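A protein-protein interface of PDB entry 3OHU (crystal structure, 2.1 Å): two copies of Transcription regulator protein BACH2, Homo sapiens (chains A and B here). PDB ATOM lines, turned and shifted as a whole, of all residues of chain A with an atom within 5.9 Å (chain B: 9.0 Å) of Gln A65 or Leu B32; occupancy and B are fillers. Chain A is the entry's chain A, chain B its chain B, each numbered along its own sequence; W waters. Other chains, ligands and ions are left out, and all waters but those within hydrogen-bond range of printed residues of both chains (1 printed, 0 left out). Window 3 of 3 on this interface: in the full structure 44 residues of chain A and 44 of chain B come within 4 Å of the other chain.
O of Ala A49 is in hydrogen-bond range of NE2 of Gln B26, 3.1 Å away.
Water W1 bridges O of Val A63 (2.5 Å) and N of Leu B32 (2.8 Å).
Among the printed residues, merely in contact across the chains: Arg A48 with Leu B32 (3.97 Å), Ala A49 with Leu B23 (3.5 Å), Ala A49 with His B47 (3.2 Å), Ala A52 with Gln B26 (3.9 Å), Ala A52 with Leu B32 (3.6 Å), Trp A59 with Ile B31 (3.7 Å), Leu A62 with Leu B32 (3.2 Å), Val A63 with Ile B31 (3.97 Å), Val A63 with Leu B32 (3.8 Å) and Gln A65 with Leu B32 (3.7 Å).
Printed residues of chain B within 4 Å of Ala A52: Gln B26 (3.9 Å) and Leu B32 (3.6 Å).
Of the printed residues of chain B, Val A63 touches Ile B31 and Leu B32.
Gln A65 touches one residue of chain B.
Printed residues of chain A within 4 Å of Ile B31: Trp A59 (3.7 Å) and Val A63 (3.97 Å).
Leu B32 touches five residues of chain A.
Arg B45 touches none of the printed residues of chain A.
Ala B46 touches none of the printed residues of chain A.
The nearest residue of chain B that does not touch Gln A65 is Cys B33 (6.3 Å).
The nearest printed residue of chain B that does not touch Arg A48 is Gln B26 (5.4 Å).
Of the 12 printed residues of chain A, 7 touch a printed residue of chain B.
Printed residues of chain A that touch a printed residue of chain B: Arg A48, Ala A49, Ala A52, Trp A59, Leu A62, Val A63 and Gln A65.
Hydrophobic or aromatic side chains of chain A that line the printed part of chain B: Ala A49, Ala A52, Trp A59 and Val A63.
Of the 20 printed residues of chain B, 5 touch a printed residue of chain A.
Hydrophobic or aromatic side chains of chain B within 4 Å of the printed part of chain A: Leu B23, Ile B31, Leu B32 and His B47.
Among the printed residues, 11 pairs touch across the chains.
Among the printed residues, no Asp or Glu carboxylate lies within 4 Å of a Lys or Arg side-chain nitrogen of the other chain.
Positions printed for both chains: 48 and 49.
The guanidinium group (NH1) of Arg A48 sits at hydrogen-bond distance from the backbone carbonyl oxygen (O) of Gln A65.
The guanidinium group (NH1) of Arg A48 lies within hydrogen-bond range of the backbone carbonyl oxygen (O) of Lys A67, 2.7 Å away.
The side-chain amide oxygen (OE1) of Gln B26 sits at hydrogen-bond distance from a ring nitrogen (NE2) of His B47, at 3.0 Å.
The backbone carbonyl oxygen (O) of Ile B31 lies within hydrogen-bond range of the side-chain sulfur (SG) of Cys B33, at 3.6 Å.
The backbone carbonyl oxygen of Leu B32 sits close to a ring nitrogen (NE2) of His B47.
The backbone NH of His B47 lies within hydrogen-bond range of the side-chain hydroxyl of Tyr B91 (2.8 Å).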
ATOM      1  N   ARG A  48      -6.712  12.176 -34.375  1.00  0.00           N
ATOM      2  CA  ARG A  48      -6.607  13.506 -33.743  1.00  0.00           C
ATOM      3  C   ARG A  48      -5.797  13.511 -32.433  1.00  0.00           C
ATOM      4  O   ARG A  48      -4.926  14.380 -32.236  1.00  0.00           O
ATOM      5  CB  ARG A  48      -7.977  14.186 -33.568  1.00  0.00           C
ATOM      6  CG  ARG A  48      -8.913  13.542 -32.555  1.00  0.00           C
ATOM      7  CD  ARG A  48     -10.347  14.101 -32.675  1.00  0.00           C
ATOM      8  NE  ARG A  48     -11.121  13.444 -33.722  1.00  0.00           N
ATOM      9  CZ  ARG A  48     -12.438  13.577 -33.875  1.00  0.00           C
ATOM     10  NH1 ARG A  48     -13.130  14.361 -33.047  1.00  0.00           N
ATOM     11  NH2 ARG A  48     -13.052  12.937 -34.855  1.00  0.00           N
ATOM     12  N   ALA A  49      -6.053  12.529 -31.567  1.00  0.00           N
ATOM     13  CA  ALA A  49      -5.286  12.419 -30.325  1.00  0.00           C
ATOM     14  C   ALA A  49      -3.780  12.343 -30.593  1.00  0.00           C
ATOM     15  O   ALA A  49      -2.976  12.966 -29.909  1.00  0.00           O
ATOM     16  CB  ALA A  49      -5.742  11.220 -29.526  1.00  0.00           C
ATOM     17  N   ALA A  52      -2.508  15.791 -31.755  1.00  0.00           N
ATOM     18  CA  ALA A  52      -2.469  16.736 -30.644  1.00  0.00           C
ATOM     19  C   ALA A  52      -1.285  16.421 -29.742  1.00  0.00           C
ATOM     20  O   ALA A  52      -0.749  17.308 -29.095  1.00  0.00           O
ATOM     21  CB  ALA A  52      -3.763  16.687 -29.854  1.00  0.00           C
ATOM     22  N   TRP A  59      -2.650  20.345 -31.272  1.00  0.00           N
ATOM     23  CA  TRP A  59      -3.289  20.357 -29.956  1.00  0.00           C
ATOM     24  C   TRP A  59      -4.342  21.477 -29.867  1.00  0.00           C
ATOM     25  O   TRP A  59      -5.492  21.222 -29.498  1.00  0.00           O
ATOM     26  CB  TRP A  59      -2.261  20.485 -28.828  1.00  0.00           C
ATOM     27  CG  TRP A  59      -2.871  20.997 -27.559  1.00  0.00           C
ATOM     28  CD1 TRP A  59      -3.188  22.300 -27.253  1.00  0.00           C
ATOM     29  CD2 TRP A  59      -3.266  20.221 -26.440  1.00  0.00           C
ATOM     30  NE1 TRP A  59      -3.747  22.375 -26.003  1.00  0.00           N
ATOM     31  CE2 TRP A  59      -3.801  21.110 -25.480  1.00  0.00           C
ATOM     32  CE3 TRP A  59      -3.206  18.855 -26.141  1.00  0.00           C
ATOM     33  CZ2 TRP A  59      -4.279  20.675 -24.255  1.00  0.00           C
ATOM     34  CZ3 TRP A  59      -3.679  18.429 -24.918  1.00  0.00           C
ATOM     35  CH2 TRP A  59      -4.207  19.331 -23.995  1.00  0.00           C
ATOM     36  N   ALA A  61      -5.662  23.309 -32.369  1.00  0.00           N
ATOM     37  CA  ALA A  61      -6.674  23.161 -33.393  1.00  0.00           C
ATOM     38  C   ALA A  61      -7.712  22.110 -33.018  1.00  0.00           C
ATOM     39  O   ALA A  61      -8.891  22.243 -33.385  1.00  0.00           O
ATOM     40  CB  ALA A  61      -6.043  22.837 -34.738  1.00  0.00           C
ATOM     41  N   LEU A  62      -7.315  21.086 -32.266  1.00  0.00           N
ATOM     42  CA  LEU A  62      -8.179  19.908 -32.162  1.00  0.00           C
ATOM     43  C   LEU A  62      -8.830  19.647 -30.822  1.00  0.00           C
ATOM     44  O   LEU A  62      -9.788  18.879 -30.755  1.00  0.00           O
ATOM     45  CB  LEU A  62      -7.487  18.637 -32.662  1.00  0.00           C
ATOM     46  CG  LEU A  62      -6.900  18.617 -34.072  1.00  0.00           C
ATOM     47  CD1 LEU A  62      -5.890  17.490 -34.180  1.00  0.00           C
ATOM     48  CD2 LEU A  62      -7.979  18.482 -35.154  1.00  0.00           C
ATOM     49  N   VAL A  63      -8.335  20.287 -29.764  1.00  0.00           N
ATOM     50  CA  VAL A  63      -8.730  19.915 -28.390  1.00  0.00           C
ATOM     51  C   VAL A  63     -10.232  19.935 -28.063  1.00  0.00           C
ATOM     52  O   VAL A  63     -10.723  19.050 -27.335  1.00  0.00           O
ATOM     53  CB  VAL A  63      -7.859  20.622 -27.302  1.00  0.00           C
ATOM     54  CG1 VAL A  63      -8.604  20.770 -25.998  1.00  0.00           C
ATOM     55  CG2 VAL A  63      -6.598  19.794 -27.059  1.00  0.00           C
ATOM     56  N   GLY A  64     -10.960  20.914 -28.586  1.00  0.00           N
ATOM     57  CA  GLY A  64     -12.420  20.951 -28.389  1.00  0.00           C
ATOM     58  C   GLY A  64     -13.256  20.066 -29.318  1.00  0.00           C
ATOM     59  O   GLY A  64     -14.472  19.946 -29.131  1.00  0.00           O
ATOM     60  N   GLN A  65     -12.610  19.444 -30.307  1.00  0.00           N
ATOM     61  CA  GLN A  65     -13.301  18.685 -31.361  1.00  0.00           C
ATOM     62  C   GLN A  65     -13.765  17.288 -30.927  1.00  0.00           C
ATOM     63  O   GLN A  65     -12.949  16.359 -30.803  1.00  0.00           O
ATOM     64  CB  GLN A  65     -12.433  18.588 -32.634  1.00  0.00           C
ATOM     65  CG  GLN A  65     -12.042  19.926 -33.245  1.00  0.00           C
ATOM     66  CD  GLN A  65     -13.241  20.836 -33.466  1.00  0.00           C
ATOM     67  OE1 GLN A  65     -14.257  20.435 -34.048  1.00  0.00           O
ATOM     68  NE2 GLN A  65     -13.135  22.065 -32.982  1.00  0.00           N
ATOM     69  N   THR A  66     -15.074  17.156 -30.719  1.00  0.00           N
ATOM     70  CA  THR A  66     -15.711  15.912 -30.273  1.00  0.00           C
ATOM     71  C   THR A  66     -16.622  15.291 -31.341  1.00  0.00           C
ATOM     72  O   THR A  66     -17.319  14.307 -31.082  1.00  0.00           O
ATOM     73  CB  THR A  66     -16.556  16.154 -29.012  1.00  0.00           C
ATOM     74  OG1 THR A  66     -17.637  17.046 -29.327  1.00  0.00           O
ATOM     75  CG2 THR A  66     -15.702  16.765 -27.904  1.00  0.00           C
ATOM     76  N   LYS A  67     -16.620  15.885 -32.532  1.00  0.00           N
ATOM     77  CA  LYS A  67     -17.377  15.382 -33.691  1.00  0.00           C
ATOM     78  C   LYS A  67     -16.773  14.070 -34.189  1.00  0.00           C
ATOM     79  O   LYS A  67     -15.567  13.876 -34.121  1.00  0.00           O
ATOM     80  CB  LYS A  67     -17.290  16.425 -34.813  1.00  0.00           C
ATOM     81  CG  LYS A  67     -18.492  16.532 -35.700  1.00  0.00           C
ATOM     82  CD  LYS A  67     -18.224  17.545 -36.818  1.00  0.00           C
ATOM     83  CE  LYS A  67     -19.295  17.473 -37.891  1.00  0.00           C
ATOM     84  NZ  LYS A  67     -19.241  16.160 -38.578  1.00  0.00           N
ATOM     85  N   LEU A  70     -14.617  14.281 -38.934  1.00  0.00           N
ATOM     86  CA  LEU A  70     -13.880  15.536 -38.812  1.00  0.00           C
ATOM     87  C   LEU A  70     -12.870  15.699 -39.933  1.00  0.00           C
ATOM     88  O   LEU A  70     -11.991  14.853 -40.108  1.00  0.00           O
ATOM     89  CB  LEU A  70     -13.166  15.600 -37.456  1.00  0.00           C
ATOM     90  CG  LEU A  70     -12.357  16.845 -37.101  1.00  0.00           C
ATOM     91  CD1 LEU A  70     -13.198  18.125 -37.061  1.00  0.00           C
ATOM     92  CD2 LEU A  70     -11.683  16.615 -35.757  1.00  0.00           C
ATOM     93  N   GLY B  22       1.650  11.643 -23.659  1.00  0.00           N
ATOM     94  CA  GLY B  22       0.665  12.630 -24.069  1.00  0.00           C
ATOM     95  C   GLY B  22      -0.725  12.040 -24.180  1.00  0.00           C
ATOM     96  O   GLY B  22      -1.688  12.653 -23.743  1.00  0.00           O
ATOM     97  N   LEU B  23      -0.832  10.842 -24.752  1.00  0.00           N
ATOM     98  CA  LEU B  23      -2.119  10.162 -24.859  1.00  0.00           C
ATOM     99  C   LEU B  23      -2.725   9.861 -23.494  1.00  0.00           C
ATOM    100  O   LEU B  23      -3.934  10.068 -23.267  1.00  0.00           O
ATOM    101  CB  LEU B  23      -2.002   8.908 -25.721  1.00  0.00           C
ATOM    102  CG  LEU B  23      -1.616   9.235 -27.175  1.00  0.00           C
ATOM    103  CD1 LEU B  23      -1.300   7.984 -28.010  1.00  0.00           C
ATOM    104  CD2 LEU B  23      -2.671  10.098 -27.855  1.00  0.00           C
ATOM    105  N   ASP B  25      -2.004  11.515 -20.655  1.00  0.00           N
ATOM    106  CA  ASP B  25      -2.386  12.801 -20.065  1.00  0.00           C
ATOM    107  C   ASP B  25      -3.799  13.184 -20.561  1.00  0.00           C
ATOM    108  O   ASP B  25      -4.635  13.623 -19.775  1.00  0.00           O
ATOM    109  CB  ASP B  25      -1.341  13.891 -20.399  1.00  0.00           C
ATOM    110  CG  ASP B  25      -1.635  15.252 -19.726  1.00  0.00           C
ATOM    111  OD1 ASP B  25      -1.773  15.325 -18.484  1.00  0.00           O
ATOM    112  OD2 ASP B  25      -1.709  16.277 -20.443  1.00  0.00           O
ATOM    113  N   GLN B  26      -4.057  12.983 -21.859  1.00  0.00           N
ATOM    114  CA  GLN B  26      -5.383  13.254 -22.449  1.00  0.00           C
ATOM    115  C   GLN B  26      -6.443  12.389 -21.771  1.00  0.00           C
ATOM    116  O   GLN B  26      -7.466  12.901 -21.323  1.00  0.00           O
ATOM    117  CB  GLN B  26      -5.384  12.993 -23.960  1.00  0.00           C
ATOM    118  CG  GLN B  26      -4.556  13.969 -24.810  1.00  0.00           C
ATOM    119  CD  GLN B  26      -4.474  13.521 -26.266  1.00  0.00           C
ATOM    120  OE1 GLN B  26      -5.285  12.713 -26.719  1.00  0.00           O
ATOM    121  NE2 GLN B  26      -3.496  14.047 -27.003  1.00  0.00           N
ATOM    122  N   ARG B  27      -6.172  11.083 -21.683  1.00  0.00           N
ATOM    123  CA  ARG B  27      -7.070  10.135 -21.021  1.00  0.00           C
ATOM    124  C   ARG B  27      -7.414  10.573 -19.604  1.00  0.00           C
ATOM    125  O   ARG B  27      -8.581  10.579 -19.201  1.00  0.00           O
ATOM    126  CB  ARG B  27      -6.458   8.732 -20.995  1.00  0.00           C
ATOM    127  CG  ARG B  27      -7.312   7.702 -20.260  1.00  0.00           C
ATOM    128  CD  ARG B  27      -6.704   6.312 -20.344  1.00  0.00           C
ATOM    129  NE  ARG B  27      -5.534   6.177 -19.476  1.00  0.00           N
ATOM    130  CZ  ARG B  27      -5.559   5.726 -18.220  1.00  0.00           C
ATOM    131  NH1 ARG B  27      -6.702   5.332 -17.659  1.00  0.00           N
ATOM    132  NH2 ARG B  27      -4.424   5.655 -17.535  1.00  0.00           N
ATOM    133  N   LYS B  28      -6.393  10.950 -18.849  1.00  0.00           N
ATOM    134  CA  LYS B  28      -6.605  11.322 -17.460  1.00  0.00           C
ATOM    135  C   LYS B  28      -7.476  12.562 -17.305  1.00  0.00           C
ATOM    136  O   LYS B  28      -8.304  12.624 -16.389  1.00  0.00           O
ATOM    137  CB  LYS B  28      -5.274  11.459 -16.738  1.00  0.00           C
ATOM    138  CG  LYS B  28      -4.655  10.093 -16.438  1.00  0.00           C
ATOM    139  CD  LYS B  28      -3.578  10.182 -15.394  1.00  0.00           C
ATOM    140  CE  LYS B  28      -2.285  10.667 -15.990  1.00  0.00           C
ATOM    141  NZ  LYS B  28      -1.234  10.587 -14.947  1.00  0.00           N
ATOM    142  N   LYS B  29      -7.294  13.521 -18.215  1.00  0.00           N
ATOM    143  CA  LYS B  29      -8.112  14.739 -18.284  1.00  0.00           C
ATOM    144  C   LYS B  29      -9.366  14.601 -19.162  1.00  0.00           C
ATOM    145  O   LYS B  29     -10.082  15.588 -19.348  1.00  0.00           O
ATOM    146  CB  LYS B  29      -7.274  15.913 -18.809  1.00  0.00           C
ATOM    147  CG  LYS B  29      -6.067  16.303 -17.962  1.00  0.00           C
ATOM    148  CD  LYS B  29      -4.957  16.867 -18.857  1.00  0.00           C
ATOM    149  CE  LYS B  29      -4.163  17.974 -18.177  1.00  0.00           C
ATOM    150  NZ  LYS B  29      -3.669  17.608 -16.818  1.00  0.00           N
ATOM    151  N   ASP B  30      -9.614  13.407 -19.719  1.00  0.00           N
ATOM    152  CA  ASP B  30     -10.771  13.156 -20.606  1.00  0.00           C
ATOM    153  C   ASP B  30     -10.800  14.152 -21.782  1.00  0.00           C
ATOM    154  O   ASP B  30     -11.844  14.736 -22.105  1.00  0.00           O
ATOM    155  CB  ASP B  30     -12.091  13.220 -19.794  1.00  0.00           C
ATOM    156  CG  ASP B  30     -13.304  12.663 -20.549  1.00  0.00           C
ATOM    157  OD1 ASP B  30     -13.182  12.184 -21.688  1.00  0.00           O
ATOM    158  OD2 ASP B  30     -14.413  12.700 -19.974  1.00  0.00           O
ATOM    159  N   ILE B  31      -9.638  14.367 -22.390  1.00  0.00           N
ATOM    160  CA  ILE B  31      -9.525  15.184 -23.588  1.00  0.00           C
ATOM    161  C   ILE B  31      -9.381  14.225 -24.747  1.00  0.00           C
ATOM    162  O   ILE B  31      -8.682  13.218 -24.643  1.00  0.00           O
ATOM    163  CB  ILE B  31      -8.279  16.108 -23.552  1.00  0.00           C
ATOM    164  CG1 ILE B  31      -8.429  17.198 -22.489  1.00  0.00           C
ATOM    165  CG2 ILE B  31      -8.045  16.785 -24.912  1.00  0.00           C
ATOM    166  CD1 ILE B  31      -7.117  17.951 -22.220  1.00  0.00           C
ATOM    167  N   LEU B  32     -10.063  14.532 -25.846  1.00  0.00           N
ATOM    168  CA  LEU B  32      -9.853  13.839 -27.116  1.00  0.00           C
ATOM    169  C   LEU B  32      -9.948  12.308 -27.099  1.00  0.00           C
ATOM    170  O   LEU B  32      -9.462  11.637 -28.030  1.00  0.00           O
ATOM    171  CB  LEU B  32      -8.536  14.296 -27.765  1.00  0.00           C
ATOM    172  CG  LEU B  32      -8.507  15.738 -28.293  1.00  0.00           C
ATOM    173  CD1 LEU B  32      -7.189  16.030 -28.950  1.00  0.00           C
ATOM    174  CD2 LEU B  32      -9.643  16.019 -29.268  1.00  0.00           C
ATOM    175  N   CYS B  33     -10.591  11.762 -26.070  1.00  0.00           N
ATOM    176  CA  CYS B  33     -10.969  10.360 -26.080  1.00  0.00           C
ATOM    177  C   CYS B  33     -12.174  10.105 -26.983  1.00  0.00           C
ATOM    178  O   CYS B  33     -12.823  11.043 -27.433  1.00  0.00           O
ATOM    179  CB  CYS B  33     -11.214   9.859 -24.663  1.00  0.00           C
ATOM    180  SG  CYS B  33      -9.697   9.905 -23.681  1.00  0.00           S
ATOM    181  N   ASP B  34     -12.472   8.836 -27.247  1.00  0.00           N
ATOM    182  CA  ASP B  34     -13.500   8.497 -28.239  1.00  0.00           C
ATOM    183  C   ASP B  34     -14.338   7.274 -27.867  1.00  0.00           C
ATOM    184  O   ASP B  34     -15.238   6.885 -28.625  1.00  0.00           O
ATOM    185  CB  ASP B  34     -12.827   8.246 -29.589  1.00  0.00           C
ATOM    186  CG  ASP B  34     -11.699   7.247 -29.473  1.00  0.00           C
ATOM    187  OD1 ASP B  34     -12.008   6.046 -29.339  1.00  0.00           O
ATOM    188  OD2 ASP B  34     -10.518   7.670 -29.478  1.00  0.00           O
ATOM    189  N   VAL B  35     -14.021   6.650 -26.729  1.00  0.00           N
ATOM    190  CA  VAL B  35     -14.824   5.543 -26.215  1.00  0.00           C
ATOM    191  C   VAL B  35     -14.941   5.573 -24.683  1.00  0.00           C
ATOM    192  O   VAL B  35     -14.032   6.016 -23.979  1.00  0.00           O
ATOM    193  CB  VAL B  35     -14.311   4.168 -26.714  1.00  0.00           C
ATOM    194  CG1 VAL B  35     -12.971   3.810 -26.085  1.00  0.00           C
ATOM    195  CG2 VAL B  35     -15.314   3.079 -26.424  1.00  0.00           C
ATOM    196  N   ARG B  45     -12.797   6.170 -19.778  1.00  0.00           N
ATOM    197  CA  ARG B  45     -12.503   6.782 -21.087  1.00  0.00           C
ATOM    198  C   ARG B  45     -11.187   6.271 -21.679  1.00  0.00           C
ATOM    199  O   ARG B  45     -10.212   6.026 -20.949  1.00  0.00           O
ATOM    200  CB  ARG B  45     -12.457   8.308 -20.992  1.00  0.00           C
ATOM    201  CG  ARG B  45     -13.742   8.959 -20.487  1.00  0.00           C
ATOM    202  CD  ARG B  45     -14.825   9.010 -21.578  1.00  0.00           C
ATOM    203  NE  ARG B  45     -14.496   9.921 -22.681  1.00  0.00           N
ATOM    204  CZ  ARG B  45     -15.114   9.926 -23.861  1.00  0.00           C
ATOM    205  NH1 ARG B  45     -16.094   9.065 -24.108  1.00  0.00           N
ATOM    206  NH2 ARG B  45     -14.747  10.796 -24.798  1.00  0.00           N
ATOM    207  N   ALA B  46     -11.165   6.127 -23.002  1.00  0.00           N
ATOM    208  CA  ALA B  46      -9.975   5.657 -23.713  1.00  0.00           C
ATOM    209  C   ALA B  46      -9.989   6.095 -25.181  1.00  0.00           C
ATOM    210  O   ALA B  46     -11.014   6.554 -25.710  1.00  0.00           O
ATOM    211  CB  ALA B  46      -9.879   4.141 -23.623  1.00  0.00           C
ATOM    212  N   HIS B  47      -8.844   5.939 -25.826  1.00  0.00           N
ATOM    213  CA  HIS B  47      -8.729   6.058 -27.268  1.00  0.00           C
ATOM    214  C   HIS B  47      -8.844   4.652 -27.827  1.00  0.00           C
ATOM    215  O   HIS B  47      -8.027   3.790 -27.515  1.00  0.00           O
ATOM    216  CB  HIS B  47      -7.368   6.658 -27.646  1.00  0.00           C
ATOM    217  CG  HIS B  47      -7.095   7.994 -27.022  1.00  0.00           C
ATOM    218  ND1 HIS B  47      -6.534   8.135 -25.770  1.00  0.00           N
ATOM    219  CD2 HIS B  47      -7.309   9.252 -27.484  1.00  0.00           C
ATOM    220  CE1 HIS B  47      -6.402   9.420 -25.491  1.00  0.00           C
ATOM    221  NE2 HIS B  47      -6.873  10.122 -26.511  1.00  0.00           N
ATOM    222  N   ARG B  48      -9.858   4.411 -28.653  1.00  0.00           N
ATOM    223  CA  ARG B  48     -10.060   3.074 -29.208  1.00  0.00           C
ATOM    224  C   ARG B  48      -8.855   2.576 -29.996  1.00  0.00           C
ATOM    225  O   ARG B  48      -8.566   1.388 -29.989  1.00  0.00           O
ATOM    226  CB  ARG B  48     -11.350   2.977 -30.031  1.00  0.00           C
ATOM    227  CG  ARG B  48     -11.309   3.669 -31.384  1.00  0.00           C
ATOM    228  CD  ARG B  48     -12.678   3.687 -32.057  1.00  0.00           C
ATOM    229  NE  ARG B  48     -13.597   4.615 -31.398  1.00  0.00           N
ATOM    230  CZ  ARG B  48     -14.820   4.922 -31.845  1.00  0.00           C
ATOM    231  NH1 ARG B  48     -15.293   4.383 -32.959  1.00  0.00           N
ATOM    232  NH2 ARG B  48     -15.580   5.768 -31.167  1.00  0.00           N
ATOM    233  N   ALA B  49      -8.154   3.493 -30.654  1.00  0.00           N
ATOM    234  CA  ALA B  49      -7.047   3.129 -31.506  1.00  0.00           C
ATOM    235  C   ALA B  49      -5.878   2.579 -30.695  1.00  0.00           C
ATOM    236  O   ALA B  49      -5.212   1.657 -31.137  1.00  0.00           O
ATOM    237  CB  ALA B  49      -6.608   4.315 -32.347  1.00  0.00           C
ATOM    238  N   VAL B  50      -5.647   3.161 -29.522  1.00  0.00           N
ATOM    239  CA  VAL B  50      -4.615   2.711 -28.608  1.00  0.00           C
ATOM    240  C   VAL B  50      -4.941   1.299 -28.087  1.00  0.00           C
ATOM    241  O   VAL B  50      -4.127   0.391 -28.213  1.00  0.00           O
ATOM    242  CB  VAL B  50      -4.446   3.696 -27.432  1.00  0.00           C
ATOM    243  CG1 VAL B  50      -3.554   3.101 -26.368  1.00  0.00           C
ATOM    244  CG2 VAL B  50      -3.869   5.024 -27.924  1.00  0.00           C
ATOM    245  N   TYR B  91      -1.172   2.377 -21.986  1.00  0.00           N
ATOM    246  CA  TYR B  91      -0.681   3.722 -22.248  1.00  0.00           C
ATOM    247  C   TYR B  91       0.773   3.936 -21.813  1.00  0.00           C
ATOM    248  O   TYR B  91       1.534   4.606 -22.539  1.00  0.00           O
ATOM    249  CB  TYR B  91      -1.606   4.754 -21.576  1.00  0.00           C
ATOM    250  CG  TYR B  91      -2.916   4.952 -22.312  1.00  0.00           C
ATOM    251  CD1 TYR B  91      -4.057   4.231 -21.966  1.00  0.00           C
ATOM    252  CD2 TYR B  91      -3.018   5.893 -23.346  1.00  0.00           C
ATOM    253  CE1 TYR B  91      -5.258   4.421 -22.648  1.00  0.00           C
ATOM    254  CE2 TYR B  91      -4.208   6.091 -24.029  1.00  0.00           C
ATOM    255  CZ  TYR B  91      -5.322   5.355 -23.676  1.00  0.00           C
ATOM    256  OH  TYR B  91      -6.495   5.560 -24.359  1.00  0.00           O
HETATM  257  O   HOH W   1     -11.543  16.844 -26.440  1.00  0.00           O
